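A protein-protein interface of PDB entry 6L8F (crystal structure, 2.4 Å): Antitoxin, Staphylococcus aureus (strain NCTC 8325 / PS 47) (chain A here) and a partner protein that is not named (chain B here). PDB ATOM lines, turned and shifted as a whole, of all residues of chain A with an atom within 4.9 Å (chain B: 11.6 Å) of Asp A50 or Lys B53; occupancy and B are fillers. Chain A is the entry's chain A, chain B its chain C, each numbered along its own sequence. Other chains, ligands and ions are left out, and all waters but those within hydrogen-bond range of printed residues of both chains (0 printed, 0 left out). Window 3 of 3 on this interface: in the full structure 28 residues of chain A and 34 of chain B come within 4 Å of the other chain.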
ATOM      1  N   SER A  30     -36.968  -7.639  16.519  1.00  0.00           N
ATOM      2  CA  SER A  30     -35.727  -7.316  15.799  1.00  0.00           C
ATOM      3  C   SER A  30     -35.950  -6.261  14.716  1.00  0.00           C
ATOM      4  O   SER A  30     -35.301  -6.283  13.669  1.00  0.00           O
ATOM      5  CB  SER A  30     -35.063  -8.566  15.207  1.00  0.00           C
ATOM      6  OG  SER A  30     -34.832  -9.545  16.209  1.00  0.00           O
ATOM      7  N   ASP A  31     -36.876  -5.335  14.956  1.00  0.00           N
ATOM      8  CA  ASP A  31     -37.163  -4.283  13.999  1.00  0.00           C
ATOM      9  C   ASP A  31     -36.179  -3.136  14.172  1.00  0.00           C
ATOM     10  O   ASP A  31     -35.454  -3.040  15.164  1.00  0.00           O
ATOM     11  CB  ASP A  31     -38.589  -3.747  14.167  1.00  0.00           C
ATOM     12  CG  ASP A  31     -39.652  -4.713  13.686  1.00  0.00           C
ATOM     13  OD1 ASP A  31     -39.334  -5.874  13.371  1.00  0.00           O
ATOM     14  OD2 ASP A  31     -40.828  -4.303  13.632  1.00  0.00           O
ATOM     15  N   MET A  46     -31.996   1.137  16.511  1.00  0.00           N
ATOM     16  CA  MET A  46     -31.911  -0.312  16.460  1.00  0.00           C
ATOM     17  C   MET A  46     -31.521  -0.796  17.842  1.00  0.00           C
ATOM     18  O   MET A  46     -31.093  -0.014  18.689  1.00  0.00           O
ATOM     19  CB  MET A  46     -30.897  -0.779  15.410  1.00  0.00           C
ATOM     20  CG  MET A  46     -29.455  -0.552  15.814  1.00  0.00           C
ATOM     21  SD  MET A  46     -28.334  -0.794  14.430  1.00  0.00           S
ATOM     22  CE  MET A  46     -28.996   0.425  13.318  1.00  0.00           C
ATOM     23  N   SER A  47     -31.666  -2.098  18.068  1.00  0.00           N
ATOM     24  CA  SER A  47     -31.280  -2.670  19.348  1.00  0.00           C
ATOM     25  C   SER A  47     -29.766  -2.615  19.517  1.00  0.00           C
ATOM     26  O   SER A  47     -29.012  -2.512  18.548  1.00  0.00           O
ATOM     27  CB  SER A  47     -31.754  -4.115  19.457  1.00  0.00           C
ATOM     28  OG  SER A  47     -31.026  -4.944  18.574  1.00  0.00           O
ATOM     29  N   GLU A  48     -29.327  -2.655  20.777  1.00  0.00           N
ATOM     30  CA  GLU A  48     -27.897  -2.690  21.058  1.00  0.00           C
ATOM     31  C   GLU A  48     -27.251  -3.960  20.508  1.00  0.00           C
ATOM     32  O   GLU A  48     -26.106  -3.917  20.037  1.00  0.00           O
ATOM     33  CB  GLU A  48     -27.656  -2.567  22.565  1.00  0.00           C
ATOM     34  CG  GLU A  48     -26.186  -2.508  22.943  1.00  0.00           C
ATOM     35  CD  GLU A  48     -25.939  -1.899  24.303  1.00  0.00           C
ATOM     36  OE1 GLU A  48     -26.745  -2.144  25.230  1.00  0.00           O
ATOM     37  OE2 GLU A  48     -24.933  -1.169  24.436  1.00  0.00           O
ATOM     38  N   SER A  49     -27.989  -5.077  20.514  1.00  0.00           N
ATOM     39  CA  SER A  49     -27.494  -6.325  19.935  1.00  0.00           C
ATOM     40  C   SER A  49     -27.242  -6.190  18.437  1.00  0.00           C
ATOM     41  O   SER A  49     -26.190  -6.603  17.935  1.00  0.00           O
ATOM     42  CB  SER A  49     -28.492  -7.453  20.200  1.00  0.00           C
ATOM     43  OG  SER A  49     -28.514  -7.807  21.570  1.00  0.00           O
ATOM     44  N   ASP A  50     -28.196  -5.598  17.712  1.00  0.00           N
ATOM     45  CA  ASP A  50     -28.062  -5.424  16.268  1.00  0.00           C
ATOM     46  C   ASP A  50     -26.933  -4.462  15.921  1.00  0.00           C
ATOM     47  O   ASP A  50     -26.203  -4.685  14.950  1.00  0.00           O
ATOM     48  CB  ASP A  50     -29.378  -4.921  15.678  1.00  0.00           C
ATOM     49  CG  ASP A  50     -30.408  -6.017  15.543  1.00  0.00           C
ATOM     50  OD1 ASP A  50     -30.006  -7.165  15.252  1.00  0.00           O
ATOM     51  OD2 ASP A  50     -31.615  -5.731  15.724  1.00  0.00           O
ATOM     52  N   TYR A  51     -26.778  -3.395  16.710  1.00  0.00           N
ATOM     53  CA  TYR A  51     -25.671  -2.463  16.520  1.00  0.00           C
ATOM     54  C   TYR A  51     -24.321  -3.138  16.737  1.00  0.00           C
ATOM     55  O   TYR A  51     -23.415  -3.002  15.904  1.00  0.00           O
ATOM     56  CB  TYR A  51     -25.820  -1.279  17.474  1.00  0.00           C
ATOM     57  CG  TYR A  51     -24.616  -0.370  17.492  1.00  0.00           C
ATOM     58  CD1 TYR A  51     -24.315   0.414  16.397  1.00  0.00           C
ATOM     59  CD2 TYR A  51     -23.783  -0.296  18.601  1.00  0.00           C
ATOM     60  CE1 TYR A  51     -23.225   1.259  16.391  1.00  0.00           C
ATOM     61  CE2 TYR A  51     -22.684   0.545  18.607  1.00  0.00           C
ATOM     62  CZ  TYR A  51     -22.411   1.322  17.495  1.00  0.00           C
ATOM     63  OH  TYR A  51     -21.325   2.172  17.473  1.00  0.00           O
ATOM     64  N   ASN A  52     -24.177  -3.872  17.850  1.00  0.00           N
ATOM     65  CA  ASN A  52     -22.938  -4.599  18.124  1.00  0.00           C
ATOM     66  C   ASN A  52     -22.674  -5.676  17.077  1.00  0.00           C
ATOM     67  O   ASN A  52     -21.524  -5.860  16.666  1.00  0.00           O
ATOM     68  CB  ASN A  52     -22.983  -5.219  19.523  1.00  0.00           C
ATOM     69  CG  ASN A  52     -22.868  -4.184  20.623  1.00  0.00           C
ATOM     70  OD1 ASN A  52     -22.256  -3.135  20.439  1.00  0.00           O
ATOM     71  ND2 ASN A  52     -23.456  -4.476  21.777  1.00  0.00           N
ATOM     72  N   SER A  53     -23.725  -6.390  16.639  1.00  0.00           N
ATOM     73  CA  SER A  53     -23.585  -7.401  15.587  1.00  0.00           C
ATOM     74  C   SER A  53     -23.097  -6.785  14.287  1.00  0.00           C
ATOM     75  O   SER A  53     -22.268  -7.371  13.578  1.00  0.00           O
ATOM     76  CB  SER A  53     -24.924  -8.090  15.330  1.00  0.00           C
ATOM     77  OG  SER A  53     -25.419  -8.723  16.494  1.00  0.00           O
ATOM     78  N   MET A  54     -23.609  -5.602  13.966  1.00  0.00           N
ATOM     79  CA  MET A  54     -23.219  -4.898  12.755  1.00  0.00           C
ATOM     80  C   MET A  54     -21.775  -4.419  12.841  1.00  0.00           C
ATOM     81  O   MET A  54     -21.007  -4.576  11.885  1.00  0.00           O
ATOM     82  CB  MET A  54     -24.182  -3.730  12.548  1.00  0.00           C
ATOM     83  CG  MET A  54     -24.144  -3.049  11.223  1.00  0.00           C
ATOM     84  SD  MET A  54     -25.592  -1.965  11.154  1.00  0.00           S
ATOM     85  CE  MET A  54     -26.893  -3.139  11.547  1.00  0.00           C
ATOM     86  N   THR A  57     -19.426  -7.449  12.661  1.00  0.00           N
ATOM     87  CA  THR A  57     -19.336  -7.944  11.293  1.00  0.00           C
ATOM     88  C   THR A  57     -18.439  -7.052  10.439  1.00  0.00           C
ATOM     89  O   THR A  57     -17.558  -7.553   9.742  1.00  0.00           O
ATOM     90  CB  THR A  57     -20.736  -8.056  10.689  1.00  0.00           C
ATOM     91  OG1 THR A  57     -21.568  -8.814  11.575  1.00  0.00           O
ATOM     92  CG2 THR A  57     -20.682  -8.763   9.341  1.00  0.00           C
ATOM     93  N   LEU B  43     -24.940 -17.721  22.841  1.00  0.00           N
ATOM     94  CA  LEU B  43     -25.156 -16.296  23.066  1.00  0.00           C
ATOM     95  C   LEU B  43     -25.033 -15.869  24.525  1.00  0.00           C
ATOM     96  O   LEU B  43     -25.386 -14.731  24.849  1.00  0.00           O
ATOM     97  CB  LEU B  43     -26.526 -15.883  22.525  1.00  0.00           C
ATOM     98  CG  LEU B  43     -26.608 -15.597  21.025  1.00  0.00           C
ATOM     99  CD1 LEU B  43     -28.049 -15.289  20.622  1.00  0.00           C
ATOM    100  CD2 LEU B  43     -25.678 -14.445  20.628  1.00  0.00           C
ATOM    101  N   LYS B  48     -18.326 -11.288  25.424  1.00  0.00           N
ATOM    102  CA  LYS B  48     -19.335 -10.502  24.727  1.00  0.00           C
ATOM    103  C   LYS B  48     -19.850 -11.229  23.485  1.00  0.00           C
ATOM    104  O   LYS B  48     -19.567 -10.787  22.364  1.00  0.00           O
ATOM    105  CB  LYS B  48     -18.778  -9.127  24.328  1.00  0.00           C
ATOM    106  CG  LYS B  48     -18.162  -8.342  25.482  1.00  0.00           C
ATOM    107  CD  LYS B  48     -19.230  -7.883  26.470  1.00  0.00           C
ATOM    108  CE  LYS B  48     -18.624  -7.128  27.648  1.00  0.00           C
ATOM    109  NZ  LYS B  48     -19.011  -7.750  28.949  1.00  0.00           N
ATOM    110  N   PRO B  49     -20.573 -12.346  23.642  1.00  0.00           N
ATOM    111  CA  PRO B  49     -21.016 -13.099  22.457  1.00  0.00           C
ATOM    112  C   PRO B  49     -22.036 -12.316  21.652  1.00  0.00           C
ATOM    113  O   PRO B  49     -22.848 -11.569  22.202  1.00  0.00           O
ATOM    114  CB  PRO B  49     -21.633 -14.370  23.055  1.00  0.00           C
ATOM    115  CG  PRO B  49     -22.068 -13.968  24.418  1.00  0.00           C
ATOM    116  CD  PRO B  49     -21.084 -12.939  24.892  1.00  0.00           C
ATOM    117  N   GLU B  50     -21.964 -12.472  20.332  1.00  0.00           N
ATOM    118  CA  GLU B  50     -22.791 -11.701  19.417  1.00  0.00           C
ATOM    119  C   GLU B  50     -23.036 -12.505  18.155  1.00  0.00           C
ATOM    120  O   GLU B  50     -22.136 -13.191  17.671  1.00  0.00           O
ATOM    121  CB  GLU B  50     -22.123 -10.373  19.045  1.00  0.00           C
ATOM    122  CG  GLU B  50     -22.475  -9.229  19.967  1.00  0.00           C
ATOM    123  CD  GLU B  50     -21.324  -8.277  20.119  1.00  0.00           C
ATOM    124  OE1 GLU B  50     -20.583  -8.101  19.123  1.00  0.00           O
ATOM    125  OE2 GLU B  50     -21.158  -7.713  21.225  1.00  0.00           O
ATOM    126  N   LYS B  51     -24.252 -12.409  17.629  1.00  0.00           N
ATOM    127  CA  LYS B  51     -24.532 -12.937  16.302  1.00  0.00           C
ATOM    128  C   LYS B  51     -23.751 -12.151  15.260  1.00  0.00           C
ATOM    129  O   LYS B  51     -23.482 -10.962  15.426  1.00  0.00           O
ATOM    130  CB  LYS B  51     -26.026 -12.837  15.977  1.00  0.00           C
ATOM    131  CG  LYS B  51     -26.931 -13.784  16.731  1.00  0.00           C
ATOM    132  CD  LYS B  51     -28.388 -13.544  16.333  1.00  0.00           C
ATOM    133  CE  LYS B  51     -29.308 -14.646  16.857  1.00  0.00           C
ATOM    134  NZ  LYS B  51     -30.493 -14.091  17.586  1.00  0.00           N
ATOM    135  N   LEU B  52     -23.388 -12.815  14.175  1.00  0.00           N
ATOM    136  CA  LEU B  52     -22.797 -12.117  13.047  1.00  0.00           C
ATOM    137  C   LEU B  52     -23.815 -12.013  11.917  1.00  0.00           C
ATOM    138  O   LEU B  52     -24.782 -12.776  11.852  1.00  0.00           O
ATOM    139  CB  LEU B  52     -21.520 -12.819  12.590  1.00  0.00           C
ATOM    140  CG  LEU B  52     -20.531 -12.897  13.754  1.00  0.00           C
ATOM    141  CD1 LEU B  52     -19.302 -13.717  13.406  1.00  0.00           C
ATOM    142  CD2 LEU B  52     -20.150 -11.494  14.207  1.00  0.00           C
ATOM    143  N   LYS B  53     -23.621 -11.035  11.049  1.00  0.00           N
ATOM    144  CA  LYS B  53     -24.572 -10.800   9.974  1.00  0.00           C
ATOM    145  C   LYS B  53     -23.857 -10.999   8.644  1.00  0.00           C
ATOM    146  O   LYS B  53     -22.739 -11.530   8.608  1.00  0.00           O
ATOM    147  CB  LYS B  53     -25.208  -9.412  10.126  1.00  0.00           C
ATOM    148  CG  LYS B  53     -26.068  -9.296  11.406  1.00  0.00           C
ATOM    149  CD  LYS B  53     -26.807  -7.957  11.515  1.00  0.00           C
ATOM    150  CE  LYS B  53     -27.698  -7.901  12.766  1.00  0.00           C
ATOM    151  NZ  LYS B  53     -28.672  -9.034  12.845  1.00  0.00           N
ATOM    152  N   SER B  54     -24.531 -10.607   7.562  1.00  0.00           N
ATOM    153  CA  SER B  54     -24.008 -10.585   6.179  1.00  0.00           C
ATOM    154  C   SER B  54     -23.626 -12.025   5.804  1.00  0.00           C
ATOM    155  O   SER B  54     -24.342 -12.966   6.177  1.00  0.00           O
ATOM    156  CB  SER B  54     -22.906  -9.537   6.096  1.00  0.00           C
ATOM    157  OG  SER B  54     -22.165  -9.636   4.901  1.00  0.00           O
ATOM    158  N   ASN B  55     -22.505 -12.267   5.122  1.00  0.00           N
ATOM    159  CA  ASN B  55     -22.154 -13.650   4.810  1.00  0.00           C
ATOM    160  C   ASN B  55     -21.601 -14.422   6.008  1.00  0.00           C
ATOM    161  O   ASN B  55     -21.282 -15.605   5.860  1.00  0.00           O
ATOM    162  CB  ASN B  55     -21.137 -13.706   3.671  1.00  0.00           C
ATOM    163  CG  ASN B  55     -19.793 -13.180   4.081  1.00  0.00           C
ATOM    164  OD1 ASN B  55     -19.692 -12.100   4.669  1.00  0.00           O
ATOM    165  ND2 ASN B  55     -18.748 -13.941   3.793  1.00  0.00           N
ATOM    166  N   LEU B  56     -21.472 -13.798   7.176  1.00  0.00           N
ATOM    167  CA  LEU B  56     -21.165 -14.511   8.405  1.00  0.00           C
ATOM    168  C   LEU B  56     -22.425 -14.919   9.168  1.00  0.00           C
ATOM    169  O   LEU B  56     -22.325 -15.310  10.334  1.00  0.00           O
ATOM    170  CB  LEU B  56     -20.255 -13.647   9.289  1.00  0.00           C
ATOM    171  CG  LEU B  56     -19.010 -13.041   8.625  1.00  0.00           C
ATOM    172  CD1 LEU B  56     -18.229 -12.139   9.581  1.00  0.00           C
ATOM    173  CD2 LEU B  56     -18.120 -14.142   8.098  1.00  0.00           C
ATOM    174  N   THR B  57     -23.602 -14.819   8.541  1.00  0.00           N
ATOM    175  CA  THR B  57     -24.862 -15.167   9.194  1.00  0.00           C
ATOM    176  C   THR B  57     -24.881 -16.651   9.550  1.00  0.00           C
ATOM    177  O   THR B  57     -24.470 -17.495   8.750  1.00  0.00           O
ATOM    178  CB  THR B  57     -26.044 -14.809   8.279  1.00  0.00           C
ATOM    179  OG1 THR B  57     -26.106 -13.384   8.122  1.00  0.00           O
ATOM    180  CG2 THR B  57     -27.381 -15.287   8.850  1.00  0.00           C
ATOM    181  N   GLY B  58     -25.305 -16.957  10.781  1.00  0.00           N
ATOM    182  CA  GLY B  58     -25.241 -18.298  11.315  1.00  0.00           C
ATOM    183  C   GLY B  58     -24.069 -18.530  12.238  1.00  0.00           C
ATOM    184  O   GLY B  58     -24.045 -19.540  12.952  1.00  0.00           O
ATOM    185  N   TYR B  59     -23.109 -17.619  12.252  1.00  0.00           N
ATOM    186  CA  TYR B  59     -21.942 -17.715  13.105  1.00  0.00           C
ATOM    187  C   TYR B  59     -21.996 -16.622  14.164  1.00  0.00           C
ATOM    188  O   TYR B  59     -22.811 -15.692  14.105  1.00  0.00           O
ATOM    189  CB  TYR B  59     -20.653 -17.642  12.268  1.00  0.00           C
ATOM    190  CG  TYR B  59     -20.342 -18.954  11.576  1.00  0.00           C
ATOM    191  CD1 TYR B  59     -21.033 -19.343  10.429  1.00  0.00           C
ATOM    192  CD2 TYR B  59     -19.375 -19.822  12.086  1.00  0.00           C
ATOM    193  CE1 TYR B  59     -20.768 -20.553   9.801  1.00  0.00           C
ATOM    194  CE2 TYR B  59     -19.100 -21.037  11.461  1.00  0.00           C
ATOM    195  CZ  TYR B  59     -19.803 -21.391  10.322  1.00  0.00           C
ATOM    196  OH  TYR B  59     -19.537 -22.593   9.699  1.00  0.00           O
ATOM    197  N   TYR B  60     -21.109 -16.758  15.142  1.00  0.00           N
ATOM    198  CA  TYR B  60     -21.083 -15.919  16.328  1.00  0.00           C
ATOM    199  C   TYR B  60     -19.640 -15.526  16.582  1.00  0.00           C
ATOM    200  O   TYR B  60     -18.717 -16.213  16.160  1.00  0.00           O
ATOM    201  CB  TYR B  60     -21.638 -16.638  17.585  1.00  0.00           C
ATOM    202  CG  TYR B  60     -23.042 -17.206  17.442  1.00  0.00           C
ATOM    203  CD1 TYR B  60     -23.256 -18.439  16.828  1.00  0.00           C
ATOM    204  CD2 TYR B  60     -24.148 -16.517  17.935  1.00  0.00           C
ATOM    205  CE1 TYR B  60     -24.523 -18.949  16.678  1.00  0.00           C
ATOM    206  CE2 TYR B  60     -25.425 -17.030  17.803  1.00  0.00           C
ATOM    207  CZ  TYR B  60     -25.602 -18.246  17.173  1.00  0.00           C
ATOM    208  OH  TYR B  60     -26.862 -18.761  17.019  1.00  0.00           O
ATOM    209  N   SER B  61     -19.441 -14.432  17.291  1.00  0.00           N
ATOM    210  CA  SER B  61     -18.100 -14.061  17.701  1.00  0.00           C
ATOM    211  C   SER B  61     -18.066 -13.866  19.205  1.00  0.00           C
ATOM    212  O   SER B  61     -19.017 -13.343  19.796  1.00  0.00           O
ATOM    213  CB  SER B  61     -17.614 -12.795  17.010  1.00  0.00           C
ATOM    214  OG  SER B  61     -18.013 -11.665  17.750  1.00  0.00           O
ATOM    215  N   ARG B  62     -16.982 -14.322  19.816  1.00  0.00           N
ATOM    216  CA  ARG B  62     -16.611 -13.939  21.165  1.00  0.00           C
ATOM    217  C   ARG B  62     -15.192 -13.389  21.134  1.00  0.00           C
ATOM    218  O   ARG B  62     -14.381 -13.751  20.274  1.00  0.00           O
ATOM    219  CB  ARG B  62     -16.697 -15.122  22.145  1.00  0.00           C
ATOM    220  CG  ARG B  62     -18.118 -15.491  22.539  1.00  0.00           C
ATOM    221  CD  ARG B  62     -18.134 -16.547  23.604  1.00  0.00           C
ATOM    222  NE  ARG B  62     -19.418 -17.231  23.671  1.00  0.00           N
ATOM    223  CZ  ARG B  62     -19.988 -17.657  24.798  1.00  0.00           C
ATOM    224  NH1 ARG B  62     -19.401 -17.447  25.976  1.00  0.00           N
ATOM    225  NH2 ARG B  62     -21.155 -18.287  24.741  1.00  0.00           N
ATOM    226  N   VAL B  71     -14.560 -17.161  16.187  1.00  0.00           N
ATOM    227  CA  VAL B  71     -15.728 -17.180  15.311  1.00  0.00           C
ATOM    228  C   VAL B  71     -16.188 -18.622  15.150  1.00  0.00           C
ATOM    229  O   VAL B  71     -15.445 -19.473  14.640  1.00  0.00           O
ATOM    230  CB  VAL B  71     -15.451 -16.537  13.943  1.00  0.00           C
ATOM    231  CG1 VAL B  71     -16.723 -16.554  13.100  1.00  0.00           C
ATOM    232  CG2 VAL B  71     -14.915 -15.109  14.115  1.00  0.00           C
ATOM    233  N   TYR B  72     -17.430 -18.881  15.537  1.00  0.00           N
ATOM    234  CA  TYR B  72     -17.866 -20.237  15.787  1.00  0.00           C
ATOM    235  C   TYR B  72     -19.347 -20.361  15.496  1.00  0.00           C
ATOM    236  O   TYR B  72     -20.083 -19.371  15.447  1.00  0.00           O
ATOM    237  CB  TYR B  72     -17.603 -20.673  17.251  1.00  0.00           C
ATOM    238  CG  TYR B  72     -18.363 -19.840  18.265  1.00  0.00           C
ATOM    239  CD1 TYR B  72     -17.861 -18.617  18.689  1.00  0.00           C
ATOM    240  CD2 TYR B  72     -19.587 -20.269  18.791  1.00  0.00           C
ATOM    241  CE1 TYR B  72     -18.549 -17.833  19.591  1.00  0.00           C
ATOM    242  CE2 TYR B  72     -20.292 -19.479  19.692  1.00  0.00           C
ATOM    243  CZ  TYR B  72     -19.758 -18.265  20.096  1.00  0.00           C
ATOM    244  OH  TYR B  72     -20.432 -17.472  21.004  1.00  0.00           O
ATOM    245  N   THR B  73     -19.784 -21.606  15.365  1.00  0.00           N
ATOM    246  CA  THR B  73     -21.201 -21.913  15.357  1.00  0.00           C
ATOM    247  C   THR B  73     -21.397 -23.190  16.161  1.00  0.00           C
ATOM    248  O   THR B  73     -20.445 -23.931  16.434  1.00  0.00           O
ATOM    249  CB  THR B  73     -21.740 -22.029  13.919  1.00  0.00           C
ATOM    250  OG1 THR B  73     -23.171 -21.974  13.936  1.00  0.00           O
ATOM    251  CG2 THR B  73     -21.285 -23.320  13.257  1.00  0.00           C
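The side-chain hydroxyl (OG) of Ser A53 lies within hydrogen-bond range of the backbone carbonyl oxygen (O) of Lys B51, at 3.1 Å.
NZ of Lys B53 lies within salt-bridge range of OD1 of Asp A50 (3.3 Å).
The side-chain hydroxyl (OG1) of Thr A57 is in hydrogen-bond range of the backbone NH (N) of Lys B53, 3.1 Å away.
The backbone carbonyl oxygen of Asn A52 lies close to the side-chain carboxylate of Glu B50 (3.5 Å).
The backbone NH (N) of Ser B61 lies within hydrogen-bond range of the backbone carbonyl oxygen (O) of Glu B50 (3.0 Å).
N of Leu B52 lies within hydrogen-bond range of O of Tyr B59 (2.9 Å).
The side-chain hydroxyl (OG) of Ser A47 is in hydrogen-bond range of the side-chain carboxylate (OD2) of Asp A50, 3.0 Å away.
ND2 of Asn A52 sits at hydrogen-bond distance from O of Glu A48 (3.2 Å).
O of Ser A49 is in hydrogen-bond range of OG of Ser A53.
O of Ser A53 lies within hydrogen-bond range of OG1 of Thr A57 (2.6 Å).
Ser A53 touches Lys B53 (CB to CE, 3.8 Å).
Leu B52 touches Thr A57.
No residue of chain B comes within 4 Å of Ser A30.
No residue of chain B comes within 4 Å of Met A46.
No residue of chain B comes within 4 Å of Ser A47.
Ser A49 touches none of the printed residues of chain B.
Of chain B, only Lys B53 comes within 4 Å of Asp A50.
Of the printed residues of chain B, Asn A52 touches Glu B50 (3.5 Å).
No residue of chain B comes within 4 Å of Met A54.
Printed residues of chain B within 4 Å of Thr A57: Leu B52 and Lys B53.
Of the printed residues of chain A, Glu B50 touches Asn A52 (3.5 Å).
Of the printed residues of chain A, Lys B51 touches Ser A53 (3.1 Å).
Printed residues of chain A within 4 Å of Leu B52: Thr A57 (3.8 Å).
Asn B55 touches none of the printed residues of chain A.
Gly B58 touches none of the printed residues of chain A.
The nearest printed residue of chain B that does not touch Thr A57 is Ser B54 (4.01 Å).
Printed residues of chain A that touch a printed residue of chain B: Asp A50, Asn A52, Ser A53 and Thr A57.
Of the 19 printed residues of chain B, 4 touch a printed residue of chain A.
Among the printed residues, Asp or Glu carboxylates within 4 Å of a Lys or Arg side-chain nitrogen of the other chain: Asp A50 with Lys B53 (3.3 Å).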
